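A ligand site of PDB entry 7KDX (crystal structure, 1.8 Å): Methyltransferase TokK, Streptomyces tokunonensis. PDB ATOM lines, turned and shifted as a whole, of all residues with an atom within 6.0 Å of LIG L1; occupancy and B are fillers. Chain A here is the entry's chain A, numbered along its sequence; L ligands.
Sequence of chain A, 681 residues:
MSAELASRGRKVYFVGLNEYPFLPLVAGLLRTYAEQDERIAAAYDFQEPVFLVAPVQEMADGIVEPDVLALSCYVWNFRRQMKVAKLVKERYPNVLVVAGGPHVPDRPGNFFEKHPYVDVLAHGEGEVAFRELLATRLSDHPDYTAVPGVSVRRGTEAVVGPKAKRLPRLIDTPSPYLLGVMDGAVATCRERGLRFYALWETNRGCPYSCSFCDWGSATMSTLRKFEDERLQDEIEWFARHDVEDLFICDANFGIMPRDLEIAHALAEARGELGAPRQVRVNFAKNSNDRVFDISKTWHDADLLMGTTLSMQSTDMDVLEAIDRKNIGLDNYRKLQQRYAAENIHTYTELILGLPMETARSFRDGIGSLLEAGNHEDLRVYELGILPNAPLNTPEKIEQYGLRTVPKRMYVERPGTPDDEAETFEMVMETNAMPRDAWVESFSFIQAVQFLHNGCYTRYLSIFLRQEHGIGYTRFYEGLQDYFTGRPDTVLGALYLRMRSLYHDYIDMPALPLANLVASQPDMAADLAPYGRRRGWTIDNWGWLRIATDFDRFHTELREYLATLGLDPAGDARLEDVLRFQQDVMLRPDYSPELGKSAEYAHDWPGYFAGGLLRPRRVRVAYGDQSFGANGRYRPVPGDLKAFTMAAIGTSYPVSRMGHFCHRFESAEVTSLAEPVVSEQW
SG of Cys 206 binds FE2 of LIG L1 (2.2 Å). SG of Cys 213 is bound to FE4 of LIG L1 (2.2 Å). N of Cys 210 lies close to S3 of LIG L1 (3.6 Å). FE1 of LIG L1 is bound by SG of Cys 210 (2.3 Å). The guanidinium group (NH1) of Arg 324 sits close to a sulfur (S2) of LIG L1 (3.6 Å). An oxygen (O2) of LG2 L2 is in salt-bridge range of the guanidinium group of Arg 324, 2.9 Å away. O of Ala 251 lies close to N1 of LG2 L2, 3.0 Å away. The side-chain amide oxygen (OD1) of Asn 252 sits close to a nitrogen (N1) of LG2 L2 (3.0 Å). A nitrogen (N5) of LG3 L3 is in hydrogen-bond range of the backbone carbonyl oxygen of Phe 212, 3.1 Å away. An oxygen (O2) of LG3 L3 is in hydrogen-bond range of the side-chain amide oxygen (OE1) of Gln 312 (2.7 Å).
SG of Cys 206 sits close to N of Tyr 208 (3.4 Å). SG of Cys 206 lies close to ND2 of Asn 252, at 3.4 Å. N of Trp 215 lies close to SG of Cys 213 (3.5 Å). The side-chain sulfur (SG) of Cys 210 sits close to the guanidinium group (NH1) of Arg 324 (3.3 Å). The side-chain amide nitrogen of Gln 312 sits close to the guanidinium group of Arg 324, at 3.4 Å. The backbone NH (N) of Lys 285 is in hydrogen-bond range of the side-chain amide oxygen (OD1) of Asn 252 (2.8 Å).
CD2 of Tyr 208 touches S4 of LIG L1, at 3.6 Å. Phe 212 touches LIG L1. CB of Trp 215 touches S1 of LIG L1, at 3.8 Å. Thr 219 touches LIG L1 (CG2 to S3, 3.8 Å). CB of Ala 251 touches S1 of LIG L1, 3.8 Å away. Lys 285 touches LIG L1. Gln 312 touches LIG L1. Hydrophobic or aromatic side chains within 4 Å of LIG L1: Tyr 208, Phe 212, Trp 215 and Ala 251. 11 residues have an atom within 4 Å of LIG L1: Cys 206, Tyr 208, Cys 210, Phe 212, Cys 213, Trp 215, Thr 219, Ala 251, Lys 285, Gln 312 and Arg 324.
N1 of LG2 L2 is bound to FE3 of LIG L1. S1 of LG2 L2 lies close to O3 of LG3 L3 (3.5 Å).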
ATOM      1  N   CYS A 206       5.041   4.194 -14.402  1.00  0.00           N
ATOM      2  CA  CYS A 206       5.798   5.353 -14.855  1.00  0.00           C
ATOM      3  C   CYS A 206       7.054   5.434 -13.996  1.00  0.00           C
ATOM      4  O   CYS A 206       6.957   5.365 -12.760  1.00  0.00           O
ATOM      5  CB  CYS A 206       5.005   6.663 -14.726  1.00  0.00           C
ATOM      6  SG  CYS A 206       6.009   8.125 -15.177  1.00  0.00           S
ATOM      7  N   PRO A 207       8.230   5.595 -14.600  1.00  0.00           N
ATOM      8  CA  PRO A 207       9.466   5.638 -13.809  1.00  0.00           C
ATOM      9  C   PRO A 207       9.699   6.967 -13.121  1.00  0.00           C
ATOM     10  O   PRO A 207      10.651   7.077 -12.332  1.00  0.00           O
ATOM     11  CB  PRO A 207      10.553   5.369 -14.859  1.00  0.00           C
ATOM     12  CG  PRO A 207       9.982   5.937 -16.119  1.00  0.00           C
ATOM     13  CD  PRO A 207       8.490   5.759 -16.047  1.00  0.00           C
ATOM     14  N   TYR A 208       8.881   7.981 -13.402  1.00  0.00           N
ATOM     15  CA  TYR A 208       9.092   9.319 -12.880  1.00  0.00           C
ATOM     16  C   TYR A 208       8.220   9.519 -11.643  1.00  0.00           C
ATOM     17  O   TYR A 208       7.663   8.565 -11.089  1.00  0.00           O
ATOM     18  CB  TYR A 208       8.850  10.337 -13.995  1.00  0.00           C
ATOM     19  CG  TYR A 208       9.607   9.944 -15.247  1.00  0.00           C
ATOM     20  CD1 TYR A 208      10.995   9.801 -15.225  1.00  0.00           C
ATOM     21  CD2 TYR A 208       8.934   9.657 -16.435  1.00  0.00           C
ATOM     22  CE1 TYR A 208      11.688   9.415 -16.351  1.00  0.00           C
ATOM     23  CE2 TYR A 208       9.638   9.281 -17.575  1.00  0.00           C
ATOM     24  CZ  TYR A 208      11.010   9.164 -17.519  1.00  0.00           C
ATOM     25  OH  TYR A 208      11.704   8.779 -18.645  1.00  0.00           O
ATOM     26  N   SER A 209       8.100  10.780 -11.181  1.00  0.00           N
ATOM     27  CA  SER A 209       7.658  11.009  -9.812  1.00  0.00           C
ATOM     28  C   SER A 209       6.868  12.302  -9.637  1.00  0.00           C
ATOM     29  O   SER A 209       6.849  12.865  -8.536  1.00  0.00           O
ATOM     30  CB  SER A 209       8.861  11.027  -8.865  1.00  0.00           C
ATOM     31  OG  SER A 209       9.862  11.883  -9.388  1.00  0.00           O
ATOM     32  N   CYS A 210       6.202  12.780 -10.689  1.00  0.00           N
ATOM     33  CA  CYS A 210       5.466  14.038 -10.579  1.00  0.00           C
ATOM     34  C   CYS A 210       4.438  13.959  -9.444  1.00  0.00           C
ATOM     35  O   CYS A 210       3.609  13.048  -9.420  1.00  0.00           O
ATOM     36  CB  CYS A 210       4.777  14.353 -11.910  1.00  0.00           C
ATOM     37  SG  CYS A 210       5.900  14.320 -13.315  1.00  0.00           S
ATOM     38  N   PHE A 212       1.764  15.480  -8.437  1.00  0.00           N
ATOM     39  CA  PHE A 212       0.319  15.581  -8.642  1.00  0.00           C
ATOM     40  C   PHE A 212      -0.295  14.311  -9.226  1.00  0.00           C
ATOM     41  O   PHE A 212      -1.525  14.184  -9.248  1.00  0.00           O
ATOM     42  CB  PHE A 212      -0.001  16.751  -9.576  1.00  0.00           C
ATOM     43  CG  PHE A 212       0.696  16.671 -10.909  1.00  0.00           C
ATOM     44  CD1 PHE A 212       0.189  15.872 -11.924  1.00  0.00           C
ATOM     45  CD2 PHE A 212       1.877  17.368 -11.131  1.00  0.00           C
ATOM     46  CE1 PHE A 212       0.841  15.774 -13.134  1.00  0.00           C
ATOM     47  CE2 PHE A 212       2.529  17.270 -12.341  1.00  0.00           C
ATOM     48  CZ  PHE A 212       2.014  16.475 -13.346  1.00  0.00           C
ATOM     49  N   CYS A 213       0.522  13.384  -9.722  1.00  0.00           N
ATOM     50  CA  CYS A 213       0.095  12.306 -10.605  1.00  0.00           C
ATOM     51  C   CYS A 213      -0.068  11.000  -9.841  1.00  0.00           C
ATOM     52  O   CYS A 213       0.590  10.750  -8.831  1.00  0.00           O
ATOM     53  CB  CYS A 213       1.122  12.135 -11.734  1.00  0.00           C
ATOM     54  SG  CYS A 213       0.637  11.083 -13.109  1.00  0.00           S
ATOM     55  N   ASP A 214      -0.974  10.142 -10.335  1.00  0.00           N
ATOM     56  CA  ASP A 214      -1.148   8.786  -9.810  1.00  0.00           C
ATOM     57  C   ASP A 214      -1.398   7.815 -10.956  1.00  0.00           C
ATOM     58  O   ASP A 214      -2.240   6.909 -10.868  1.00  0.00           O
ATOM     59  CB  ASP A 214      -2.286   8.735  -8.797  1.00  0.00           C
ATOM     60  CG  ASP A 214      -2.295   7.434  -7.985  1.00  0.00           C
ATOM     61  OD1 ASP A 214      -1.249   6.749  -7.938  1.00  0.00           O
ATOM     62  OD2 ASP A 214      -3.359   7.099  -7.410  1.00  0.00           O
ATOM     63  N   TRP A 215      -0.651   7.979 -12.051  1.00  0.00           N
ATOM     64  CA  TRP A 215      -0.889   7.252 -13.296  1.00  0.00           C
ATOM     65  C   TRP A 215      -0.858   5.749 -13.080  1.00  0.00           C
ATOM     66  O   TRP A 215       0.176   5.192 -12.691  1.00  0.00           O
ATOM     67  CB  TRP A 215       0.151   7.648 -14.329  1.00  0.00           C
ATOM     68  CG  TRP A 215      -0.256   7.384 -15.739  1.00  0.00           C
ATOM     69  CD1 TRP A 215       0.055   6.305 -16.504  1.00  0.00           C
ATOM     70  CD2 TRP A 215      -1.062   8.240 -16.552  1.00  0.00           C
ATOM     71  NE1 TRP A 215      -0.509   6.431 -17.751  1.00  0.00           N
ATOM     72  CE2 TRP A 215      -1.200   7.608 -17.802  1.00  0.00           C
ATOM     73  CE3 TRP A 215      -1.689   9.470 -16.351  1.00  0.00           C
ATOM     74  CZ2 TRP A 215      -1.930   8.172 -18.846  1.00  0.00           C
ATOM     75  CZ3 TRP A 215      -2.422  10.026 -17.374  1.00  0.00           C
ATOM     76  CH2 TRP A 215      -2.536   9.373 -18.605  1.00  0.00           C
ATOM     77  N   THR A 219       3.069   5.252 -10.414  1.00  0.00           N
ATOM     78  CA  THR A 219       4.204   6.153 -10.596  1.00  0.00           C
ATOM     79  C   THR A 219       5.349   5.710  -9.681  1.00  0.00           C
ATOM     80  O   THR A 219       5.165   4.913  -8.758  1.00  0.00           O
ATOM     81  CB  THR A 219       3.829   7.609 -10.297  1.00  0.00           C
ATOM     82  OG1 THR A 219       3.488   7.740  -8.902  1.00  0.00           O
ATOM     83  CG2 THR A 219       2.655   8.055 -11.160  1.00  0.00           C
ATOM     84  N   ALA A 251       2.046   5.312 -19.799  1.00  0.00           N
ATOM     85  CA  ALA A 251       2.430   6.632 -19.300  1.00  0.00           C
ATOM     86  C   ALA A 251       3.352   7.363 -20.260  1.00  0.00           C
ATOM     87  O   ALA A 251       3.299   8.595 -20.345  1.00  0.00           O
ATOM     88  CB  ALA A 251       3.103   6.501 -17.932  1.00  0.00           C
ATOM     89  N   ASN A 252       4.214   6.632 -20.990  1.00  0.00           N
ATOM     90  CA  ASN A 252       5.298   7.255 -21.743  1.00  0.00           C
ATOM     91  C   ASN A 252       5.532   6.497 -23.048  1.00  0.00           C
ATOM     92  O   ASN A 252       6.587   5.902 -23.260  1.00  0.00           O
ATOM     93  CB  ASN A 252       6.601   7.289 -20.922  1.00  0.00           C
ATOM     94  CG  ASN A 252       6.533   8.222 -19.744  1.00  0.00           C
ATOM     95  OD1 ASN A 252       6.703   9.437 -19.898  1.00  0.00           O
ATOM     96  ND2 ASN A 252       6.307   7.674 -18.563  1.00  0.00           N
ATOM     97  N   LYS A 285       7.678  11.487 -21.582  1.00  0.00           N
ATOM     98  CA  LYS A 285       8.146  12.772 -21.057  1.00  0.00           C
ATOM     99  C   LYS A 285       9.494  13.156 -21.639  1.00  0.00           C
ATOM    100  O   LYS A 285       9.690  14.291 -22.093  1.00  0.00           O
ATOM    101  CB  LYS A 285       8.234  12.704 -19.524  1.00  0.00           C
ATOM    102  CG  LYS A 285       8.645  14.036 -18.883  1.00  0.00           C
ATOM    103  CD  LYS A 285       8.645  13.959 -17.352  1.00  0.00           C
ATOM    104  CE  LYS A 285       9.796  13.129 -16.813  1.00  0.00           C
ATOM    105  NZ  LYS A 285      11.120  13.766 -17.066  1.00  0.00           N
ATOM    106  N   GLN A 312       3.557  20.782 -17.635  1.00  0.00           N
ATOM    107  CA  GLN A 312       2.879  21.055 -16.374  1.00  0.00           C
ATOM    108  C   GLN A 312       3.224  22.453 -15.881  1.00  0.00           C
ATOM    109  O   GLN A 312       2.321  23.241 -15.555  1.00  0.00           O
ATOM    110  CB  GLN A 312       3.206  19.986 -15.313  1.00  0.00           C
ATOM    111  CG  GLN A 312       3.404  18.553 -15.843  1.00  0.00           C
ATOM    112  CD  GLN A 312       2.231  18.015 -16.639  1.00  0.00           C
ATOM    113  OE1 GLN A 312       1.177  18.635 -16.734  1.00  0.00           O
ATOM    114  NE2 GLN A 312       2.413  16.831 -17.217  1.00  0.00           N
ATOM    115  N   ARG A 324       9.642  17.123 -10.871  1.00  0.00           N
ATOM    116  CA  ARG A 324       9.570  16.911 -12.305  1.00  0.00           C
ATOM    117  C   ARG A 324      10.700  17.641 -12.996  1.00  0.00           C
ATOM    118  O   ARG A 324      10.967  18.816 -12.707  1.00  0.00           O
ATOM    119  CB  ARG A 324       8.217  17.382 -12.864  1.00  0.00           C
ATOM    120  CG  ARG A 324       8.100  17.157 -14.368  1.00  0.00           C
ATOM    121  CD  ARG A 324       6.754  17.611 -14.904  1.00  0.00           C
ATOM    122  NE  ARG A 324       6.711  17.499 -16.365  1.00  0.00           N
ATOM    123  CZ  ARG A 324       6.073  16.530 -17.025  1.00  0.00           C
ATOM    124  NH1 ARG A 324       5.410  15.591 -16.372  1.00  0.00           N
ATOM    125  NH2 ARG A 324       6.105  16.519 -18.349  1.00  0.00           N
HETATM  126 FE1  LIG L   1       4.829  12.624 -14.479  1.00  0.00          FE
HETATM  127 FE2  LIG L   1       4.780   9.981 -15.093  1.00  0.00          FE
HETATM  128 FE3  LIG L   1       3.634  11.857 -16.882  1.00  0.00          FE
HETATM  129 FE4  LIG L   1       2.461  11.259 -14.414  1.00  0.00          FE
HETATM  130  S1  LIG L   1       2.722   9.836 -16.146  1.00  0.00           S
HETATM  131  S2  LIG L   1       2.803  13.345 -15.339  1.00  0.00           S
HETATM  132  S3  LIG L   1       4.309  10.897 -13.087  1.00  0.00           S
HETATM  133  S4  LIG L   1       5.889  11.645 -16.222  1.00  0.00           S
HETATM  134  N1  LG2 L   2       4.348  11.099 -18.982  1.00  0.00           N
HETATM  135  C1  LG2 L   2       4.295  12.133 -20.014  1.00  0.00           C
HETATM  136  C2  LG2 L   2       4.566  13.489 -19.392  1.00  0.00           C
HETATM  137  O1  LG2 L   2       4.325  13.685 -18.191  1.00  0.00           O
HETATM  138  C3  LG2 L   2       2.935  12.147 -20.719  1.00  0.00           C
HETATM  139  C4  LG2 L   2       1.849  12.913 -19.968  1.00  0.00           C
HETATM  140  S1  LG2 L   2       1.381  12.217 -18.359  1.00  0.00           S
HETATM  141  C5  LG2 L   2       0.804  10.592 -18.864  1.00  0.00           C
HETATM  142  O2  LG2 L   2       5.034  14.419 -20.058  1.00  0.00           O
HETATM  143  N1  LG3 L   3      -4.656  17.402 -11.857  1.00  0.00           N
HETATM  144  C1  LG3 L   3      -4.697  17.967 -13.073  1.00  0.00           C
HETATM  145  N2  LG3 L   3      -4.153  17.533 -14.216  1.00  0.00           N
HETATM  146  C2  LG3 L   3      -3.507  16.374 -14.045  1.00  0.00           C
HETATM  147  N3  LG3 L   3      -2.854  15.636 -14.993  1.00  0.00           N
HETATM  148  C3  LG3 L   3      -2.378  14.527 -14.340  1.00  0.00           C
HETATM  149  N4  LG3 L   3      -2.664  14.498 -13.065  1.00  0.00           N
HETATM  150  C4  LG3 L   3      -3.382  15.670 -12.857  1.00  0.00           C
HETATM  151  C5  LG3 L   3      -3.983  16.230 -11.718  1.00  0.00           C
HETATM  152  N5  LG3 L   3      -3.896  15.663 -10.511  1.00  0.00           N
HETATM  153  C6  LG3 L   3      -2.666  15.972 -16.398  1.00  0.00           C
HETATM  154  C7  LG3 L   3      -1.219  16.335 -16.764  1.00  0.00           C
HETATM  155  C8  LG3 L   3      -0.774  15.131 -17.607  1.00  0.00           C
HETATM  156  C9  LG3 L   3      -2.081  14.729 -18.262  1.00  0.00           C
HETATM  157  C10 LG3 L   3      -2.121  13.318 -18.815  1.00  0.00           C
HETATM  158  O1  LG3 L   3      -3.043  14.857 -17.196  1.00  0.00           O
HETATM  159  O2  LG3 L   3      -1.220  17.556 -17.493  1.00  0.00           O
HETATM  160  O3  LG3 L   3       0.191  15.457 -18.587  1.00  0.00           O
